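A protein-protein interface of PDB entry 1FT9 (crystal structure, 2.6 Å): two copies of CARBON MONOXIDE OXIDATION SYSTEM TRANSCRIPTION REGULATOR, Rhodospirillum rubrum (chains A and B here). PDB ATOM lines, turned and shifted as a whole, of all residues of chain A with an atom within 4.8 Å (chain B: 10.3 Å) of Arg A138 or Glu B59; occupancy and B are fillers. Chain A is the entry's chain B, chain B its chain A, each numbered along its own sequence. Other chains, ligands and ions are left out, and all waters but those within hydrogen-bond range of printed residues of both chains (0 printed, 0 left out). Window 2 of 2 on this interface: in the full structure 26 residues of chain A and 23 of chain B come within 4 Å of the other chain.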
ATOM      1  N   MET A 131      14.515  21.757  -4.192  1.00  0.00           N
ATOM      2  CA  MET A 131      13.733  20.619  -3.736  1.00  0.00           C
ATOM      3  C   MET A 131      12.231  20.876  -3.696  1.00  0.00           C
ATOM      4  O   MET A 131      11.442  19.988  -4.014  1.00  0.00           O
ATOM      5  CB  MET A 131      14.227  20.174  -2.364  1.00  0.00           C
ATOM      6  CG  MET A 131      15.708  19.908  -2.338  1.00  0.00           C
ATOM      7  SD  MET A 131      16.148  18.862  -0.970  1.00  0.00           S
ATOM      8  CE  MET A 131      16.119  20.057   0.396  1.00  0.00           C
ATOM      9  N   ASP A 134      10.980  20.666  -7.175  1.00  0.00           N
ATOM     10  CA  ASP A 134      10.925  19.289  -7.657  1.00  0.00           C
ATOM     11  C   ASP A 134       9.714  18.528  -7.119  1.00  0.00           C
ATOM     12  O   ASP A 134       9.001  17.881  -7.879  1.00  0.00           O
ATOM     13  CB  ASP A 134      12.209  18.551  -7.274  1.00  0.00           C
ATOM     14  CG  ASP A 134      13.424  19.077  -8.015  1.00  0.00           C
ATOM     15  OD1 ASP A 134      13.512  20.308  -8.222  1.00  0.00           O
ATOM     16  OD2 ASP A 134      14.299  18.265  -8.385  1.00  0.00           O
ATOM     17  N   ILE A 135       9.473  18.605  -5.815  1.00  0.00           N
ATOM     18  CA  ILE A 135       8.335  17.898  -5.236  1.00  0.00           C
ATOM     19  C   ILE A 135       7.023  18.348  -5.870  1.00  0.00           C
ATOM     20  O   ILE A 135       6.083  17.564  -5.985  1.00  0.00           O
ATOM     21  CB  ILE A 135       8.236  18.115  -3.718  1.00  0.00           C
ATOM     22  CG1 ILE A 135       7.150  17.209  -3.142  1.00  0.00           C
ATOM     23  CG2 ILE A 135       7.912  19.571  -3.419  1.00  0.00           C
ATOM     24  CD1 ILE A 135       6.991  17.320  -1.652  1.00  0.00           C
ATOM     25  N   LYS A 136       6.958  19.613  -6.273  1.00  0.00           N
ATOM     26  CA  LYS A 136       5.756  20.146  -6.902  1.00  0.00           C
ATOM     27  C   LYS A 136       5.477  19.421  -8.209  1.00  0.00           C
ATOM     28  O   LYS A 136       4.345  19.013  -8.475  1.00  0.00           O
ATOM     29  CB  LYS A 136       5.912  21.633  -7.191  1.00  0.00           C
ATOM     30  CG  LYS A 136       5.408  22.559  -6.105  1.00  0.00           C
ATOM     31  CD  LYS A 136       5.526  23.989  -6.595  1.00  0.00           C
ATOM     32  CE  LYS A 136       5.026  24.977  -5.574  1.00  0.00           C
ATOM     33  NZ  LYS A 136       5.219  26.379  -6.038  1.00  0.00           N
ATOM     34  N   GLN A 137       6.520  19.276  -9.024  1.00  0.00           N
ATOM     35  CA  GLN A 137       6.409  18.602 -10.310  1.00  0.00           C
ATOM     36  C   GLN A 137       5.972  17.165 -10.091  1.00  0.00           C
ATOM     37  O   GLN A 137       5.238  16.595 -10.894  1.00  0.00           O
ATOM     38  CB  GLN A 137       7.753  18.612 -11.028  1.00  0.00           C
ATOM     39  CG  GLN A 137       8.365  19.983 -11.184  1.00  0.00           C
ATOM     40  CD  GLN A 137       9.723  19.926 -11.845  1.00  0.00           C
ATOM     41  OE1 GLN A 137      10.647  19.279 -11.344  1.00  0.00           O
ATOM     42  NE2 GLN A 137       9.855  20.604 -12.981  1.00  0.00           N
ATOM     43  N   ARG A 138       6.441  16.586  -8.993  1.00  0.00           N
ATOM     44  CA  ARG A 138       6.112  15.214  -8.639  1.00  0.00           C
ATOM     45  C   ARG A 138       4.607  15.156  -8.430  1.00  0.00           C
ATOM     46  O   ARG A 138       3.920  14.314  -9.002  1.00  0.00           O
ATOM     47  CB  ARG A 138       6.832  14.825  -7.345  1.00  0.00           C
ATOM     48  CG  ARG A 138       6.949  13.328  -7.095  1.00  0.00           C
ATOM     49  CD  ARG A 138       8.229  12.775  -7.692  1.00  0.00           C
ATOM     50  NE  ARG A 138       9.395  13.562  -7.290  1.00  0.00           N
ATOM     51  CZ  ARG A 138       9.761  13.786  -6.029  1.00  0.00           C
ATOM     52  NH1 ARG A 138       9.056  13.283  -5.020  1.00  0.00           N
ATOM     53  NH2 ARG A 138      10.840  14.518  -5.775  1.00  0.00           N
ATOM     54  N   ILE A 139       4.104  16.068  -7.606  1.00  0.00           N
ATOM     55  CA  ILE A 139       2.681  16.129  -7.320  1.00  0.00           C
ATOM     56  C   ILE A 139       1.942  16.536  -8.588  1.00  0.00           C
ATOM     57  O   ILE A 139       0.781  16.178  -8.778  1.00  0.00           O
ATOM     58  CB  ILE A 139       2.372  17.141  -6.192  1.00  0.00           C
ATOM     59  CG1 ILE A 139       3.050  16.694  -4.894  1.00  0.00           C
ATOM     60  CG2 ILE A 139       0.869  17.240  -5.978  1.00  0.00           C
ATOM     61  CD1 ILE A 139       2.768  17.589  -3.705  1.00  0.00           C
ATOM     62  N   ALA A 140       2.620  17.285  -9.452  1.00  0.00           N
ATOM     63  CA  ALA A 140       2.024  17.720 -10.711  1.00  0.00           C
ATOM     64  C   ALA A 140       1.811  16.484 -11.577  1.00  0.00           C
ATOM     65  O   ALA A 140       0.686  16.177 -11.975  1.00  0.00           O
ATOM     66  CB  ALA A 140       2.946  18.701 -11.424  1.00  0.00           C
ATOM     67  N   GLY A 141       2.906  15.783 -11.856  1.00  0.00           N
ATOM     68  CA  GLY A 141       2.839  14.579 -12.659  1.00  0.00           C
ATOM     69  C   GLY A 141       1.928  13.542 -12.034  1.00  0.00           C
ATOM     70  O   GLY A 141       1.288  12.770 -12.743  1.00  0.00           O
ATOM     71  N   PHE A 142       1.865  13.514 -10.705  1.00  0.00           N
ATOM     72  CA  PHE A 142       1.007  12.556 -10.019  1.00  0.00           C
ATOM     73  C   PHE A 142      -0.445  12.754 -10.445  1.00  0.00           C
ATOM     74  O   PHE A 142      -1.126  11.802 -10.832  1.00  0.00           O
ATOM     75  CB  PHE A 142       1.102  12.724  -8.504  1.00  0.00           C
ATOM     76  CG  PHE A 142       0.186  11.811  -7.746  1.00  0.00           C
ATOM     77  CD1 PHE A 142       0.480  10.455  -7.623  1.00  0.00           C
ATOM     78  CD2 PHE A 142      -1.003  12.292  -7.202  1.00  0.00           C
ATOM     79  CE1 PHE A 142      -0.399   9.591  -6.974  1.00  0.00           C
ATOM     80  CE2 PHE A 142      -1.892  11.438  -6.553  1.00  0.00           C
ATOM     81  CZ  PHE A 142      -1.590  10.084  -6.438  1.00  0.00           C
ATOM     82  N   ILE A 173       3.859   9.483  -3.715  1.00  0.00           N
ATOM     83  CA  ILE A 173       4.864  10.418  -4.218  1.00  0.00           C
ATOM     84  C   ILE A 173       6.225  10.121  -3.607  1.00  0.00           C
ATOM     85  O   ILE A 173       7.253  10.533  -4.137  1.00  0.00           O
ATOM     86  CB  ILE A 173       4.470  11.880  -3.885  1.00  0.00           C
ATOM     87  CG1 ILE A 173       3.268  12.293  -4.732  1.00  0.00           C
ATOM     88  CG2 ILE A 173       5.638  12.820  -4.116  1.00  0.00           C
ATOM     89  CD1 ILE A 173       3.495  12.148  -6.216  1.00  0.00           C
ATOM     90  N   LEU B  56      21.117  18.101   5.703  1.00  0.00           N
ATOM     91  CA  LEU B  56      19.781  18.601   5.431  1.00  0.00           C
ATOM     92  C   LEU B  56      19.072  17.383   4.843  1.00  0.00           C
ATOM     93  O   LEU B  56      19.729  16.431   4.413  1.00  0.00           O
ATOM     94  CB  LEU B  56      19.842  19.726   4.395  1.00  0.00           C
ATOM     95  CG  LEU B  56      20.622  20.983   4.786  1.00  0.00           C
ATOM     96  CD1 LEU B  56      20.870  21.849   3.561  1.00  0.00           C
ATOM     97  CD2 LEU B  56      19.845  21.743   5.849  1.00  0.00           C
ATOM     98  N   VAL B  57      17.744  17.390   4.827  1.00  0.00           N
ATOM     99  CA  VAL B  57      17.014  16.259   4.270  1.00  0.00           C
ATOM    100  C   VAL B  57      15.904  16.729   3.344  1.00  0.00           C
ATOM    101  O   VAL B  57      15.410  17.848   3.473  1.00  0.00           O
ATOM    102  CB  VAL B  57      16.411  15.377   5.385  1.00  0.00           C
ATOM    103  CG1 VAL B  57      15.708  14.172   4.774  1.00  0.00           C
ATOM    104  CG2 VAL B  57      17.510  14.915   6.330  1.00  0.00           C
ATOM    105  N   GLY B  58      15.526  15.869   2.402  1.00  0.00           N
ATOM    106  CA  GLY B  58      14.474  16.203   1.463  1.00  0.00           C
ATOM    107  C   GLY B  58      14.512  15.342   0.215  1.00  0.00           C
ATOM    108  O   GLY B  58      15.583  14.918  -0.222  1.00  0.00           O
ATOM    109  N   GLU B  59      13.338  15.083  -0.358  1.00  0.00           N
ATOM    110  CA  GLU B  59      13.218  14.273  -1.571  1.00  0.00           C
ATOM    111  C   GLU B  59      13.479  12.790  -1.297  1.00  0.00           C
ATOM    112  O   GLU B  59      14.108  12.109  -2.112  1.00  0.00           O
ATOM    113  CB  GLU B  59      14.197  14.770  -2.649  1.00  0.00           C
ATOM    114  CG  GLU B  59      14.046  16.244  -3.039  1.00  0.00           C
ATOM    115  CD  GLU B  59      12.777  16.531  -3.830  1.00  0.00           C
ATOM    116  OE1 GLU B  59      11.670  16.242  -3.322  1.00  0.00           O
ATOM    117  OE2 GLU B  59      12.886  17.049  -4.965  1.00  0.00           O
ATOM    118  N   GLU B  60      12.998  12.298  -0.154  1.00  0.00           N
ATOM    119  CA  GLU B  60      13.190  10.894   0.221  1.00  0.00           C
ATOM    120  C   GLU B  60      14.675  10.602   0.476  1.00  0.00           C
ATOM    121  O   GLU B  60      15.044   9.515   0.923  1.00  0.00           O
ATOM    122  CB  GLU B  60      12.644   9.982  -0.896  1.00  0.00           C
ATOM    123  CG  GLU B  60      13.225   8.567  -0.948  1.00  0.00           C
ATOM    124  CD  GLU B  60      12.768   7.682   0.198  1.00  0.00           C
ATOM    125  OE1 GLU B  60      12.867   8.111   1.368  1.00  0.00           O
ATOM    126  OE2 GLU B  60      12.317   6.548  -0.077  1.00  0.00           O
ATOM    127  N   ARG B  61      15.518  11.595   0.214  1.00  0.00           N
ATOM    128  CA  ARG B  61      16.960  11.454   0.376  1.00  0.00           C
ATOM    129  C   ARG B  61      17.576  12.443   1.363  1.00  0.00           C
ATOM    130  O   ARG B  61      17.117  13.578   1.490  1.00  0.00           O
ATOM    131  CB  ARG B  61      17.622  11.608  -0.998  1.00  0.00           C
ATOM    132  CG  ARG B  61      19.056  12.093  -0.973  1.00  0.00           C
ATOM    133  CD  ARG B  61      19.577  12.297  -2.382  1.00  0.00           C
ATOM    134  NE  ARG B  61      20.929  12.845  -2.388  1.00  0.00           N
ATOM    135  CZ  ARG B  61      21.672  12.994  -3.480  1.00  0.00           C
ATOM    136  NH1 ARG B  61      21.198  12.635  -4.668  1.00  0.00           N
ATOM    137  NH2 ARG B  61      22.892  13.505  -3.386  1.00  0.00           N
ATOM    138  N   GLU B  62      18.615  12.000   2.066  1.00  0.00           N
ATOM    139  CA  GLU B  62      19.314  12.857   3.016  1.00  0.00           C
ATOM    140  C   GLU B  62      20.610  13.339   2.373  1.00  0.00           C
ATOM    141  O   GLU B  62      21.396  12.540   1.858  1.00  0.00           O
ATOM    142  CB  GLU B  62      19.636  12.102   4.312  1.00  0.00           C
ATOM    143  CG  GLU B  62      18.428  11.796   5.183  1.00  0.00           C
ATOM    144  CD  GLU B  62      18.809  11.222   6.541  1.00  0.00           C
ATOM    145  OE1 GLU B  62      19.492  10.175   6.581  1.00  0.00           O
ATOM    146  OE2 GLU B  62      18.422  11.817   7.572  1.00  0.00           O
ATOM    147  N   ILE B  63      20.822  14.651   2.393  1.00  0.00           N
ATOM    148  CA  ILE B  63      22.025  15.235   1.815  1.00  0.00           C
ATOM    149  C   ILE B  63      23.072  15.502   2.883  1.00  0.00           C
ATOM    150  O   ILE B  63      22.945  16.435   3.683  1.00  0.00           O
ATOM    151  CB  ILE B  63      21.729  16.563   1.060  1.00  0.00           C
ATOM    152  CG1 ILE B  63      20.721  17.413   1.843  1.00  0.00           C
ATOM    153  CG2 ILE B  63      21.232  16.258  -0.353  1.00  0.00           C
ATOM    154  CD1 ILE B  63      19.267  16.974   1.694  1.00  0.00           C
ATOM    155  N   THR B 126      26.177  20.264  -3.429  1.00  0.00           N
ATOM    156  CA  THR B 126      24.811  19.749  -3.404  1.00  0.00           C
ATOM    157  C   THR B 126      23.913  20.451  -4.434  1.00  0.00           C
ATOM    158  O   THR B 126      23.056  19.818  -5.054  1.00  0.00           O
ATOM    159  CB  THR B 126      24.206  19.873  -1.986  1.00  0.00           C
ATOM    160  OG1 THR B 126      24.774  18.862  -1.140  1.00  0.00           O
ATOM    161  CG2 THR B 126      22.690  19.688  -2.019  1.00  0.00           C
ATOM    162  N   LEU B 130      22.178  18.963  -8.159  1.00  0.00           N
ATOM    163  CA  LEU B 130      20.788  19.091  -8.574  1.00  0.00           C
ATOM    164  C   LEU B 130      20.655  19.720  -9.947  1.00  0.00           C
ATOM    165  O   LEU B 130      19.890  19.254 -10.775  1.00  0.00           O
ATOM    166  CB  LEU B 130      20.001  19.903  -7.545  1.00  0.00           C
ATOM    167  CG  LEU B 130      19.541  19.151  -6.294  1.00  0.00           C
ATOM    168  CD1 LEU B 130      20.673  18.306  -5.756  1.00  0.00           C
ATOM    169  CD2 LEU B 130      19.069  20.139  -5.245  1.00  0.00           C
ATOM    170  N   HIS B 133      21.709  16.726 -12.183  1.00  0.00           N
ATOM    171  CA  HIS B 133      21.335  15.342 -11.889  1.00  0.00           C
ATOM    172  C   HIS B 133      21.273  14.454 -13.130  1.00  0.00           C
ATOM    173  O   HIS B 133      21.876  13.380 -13.161  1.00  0.00           O
ATOM    174  CB  HIS B 133      19.979  15.297 -11.177  1.00  0.00           C
ATOM    175  CG  HIS B 133      19.498  13.908 -10.871  1.00  0.00           C
ATOM    176  ND1 HIS B 133      20.248  12.997 -10.155  1.00  0.00           N
ATOM    177  CD2 HIS B 133      18.325  13.287 -11.152  1.00  0.00           C
ATOM    178  CE1 HIS B 133      19.559  11.879 -10.007  1.00  0.00           C
ATOM    179  NE2 HIS B 133      18.389  12.030 -10.602  1.00  0.00           N
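Asp A134 touches one residue of chain B.
Of chain B, only Glu B59 comes within 4 Å of Arg A138.
No residue of chain B comes within 4 Å of Ile A139.
No residue of chain B comes within 4 Å of Gly A141.
No residue of chain B comes within 4 Å of Ile A173.
Of the printed residues of chain A, Val B57 touches Met A131.
Printed residues of chain A within 4 Å of Gly B58: Met A131.
Glu B59 touches just these residues of chain A: Met A131 (3.4 Å), Asp A134 (2.8 Å), Ile A135 (3.8 Å) and Arg A138 (3.1 Å).
Ile B63 touches none of the printed residues of chain A.
The nearest printed residue of chain A that does not touch Glu B59 is Lys A136 (6.5 Å).
The nearest printed residue of chain A that does not touch Val B57 is Ile A135 (9.9 Å).
No position is printed for both chains.
The backbone carbonyl oxygen (O) of Ile A173 is in hydrogen-bond range of the guanidinium group (NH1) of Arg A138, 3.4 Å away.
The side-chain carboxylate of Glu B59 sits close to the backbone carbonyl oxygen of Met A131 (3.4 Å).
The guanidinium group (NH2) of Arg A138 lies within salt-bridge range of the side-chain carboxylate (OE1) of Glu B59 (3.1 Å).
O of Val B57 touches CE of Met A131, 3.9 Å away.
Gly B58 touches Met A131.
Asp A134 touches Glu B59 (CB to OE2, 2.8 Å).
OE2 of Glu B59 touches N of Ile A135, at 3.8 Å.
Printed residues of chain B that touch a printed residue of chain A: Val B57, Gly B58 and Glu B59.
Along chain B the printed residues that touch a printed residue of chain A span positions 57 to 59.
Of the 11 printed residues of chain A, 4 touch a printed residue of chain B.
Among the printed residues, Asp or Glu carboxylates within 4 Å of a Lys or Arg side-chain nitrogen of the other chain: Arg A138 with Glu B59 (3.1 Å).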
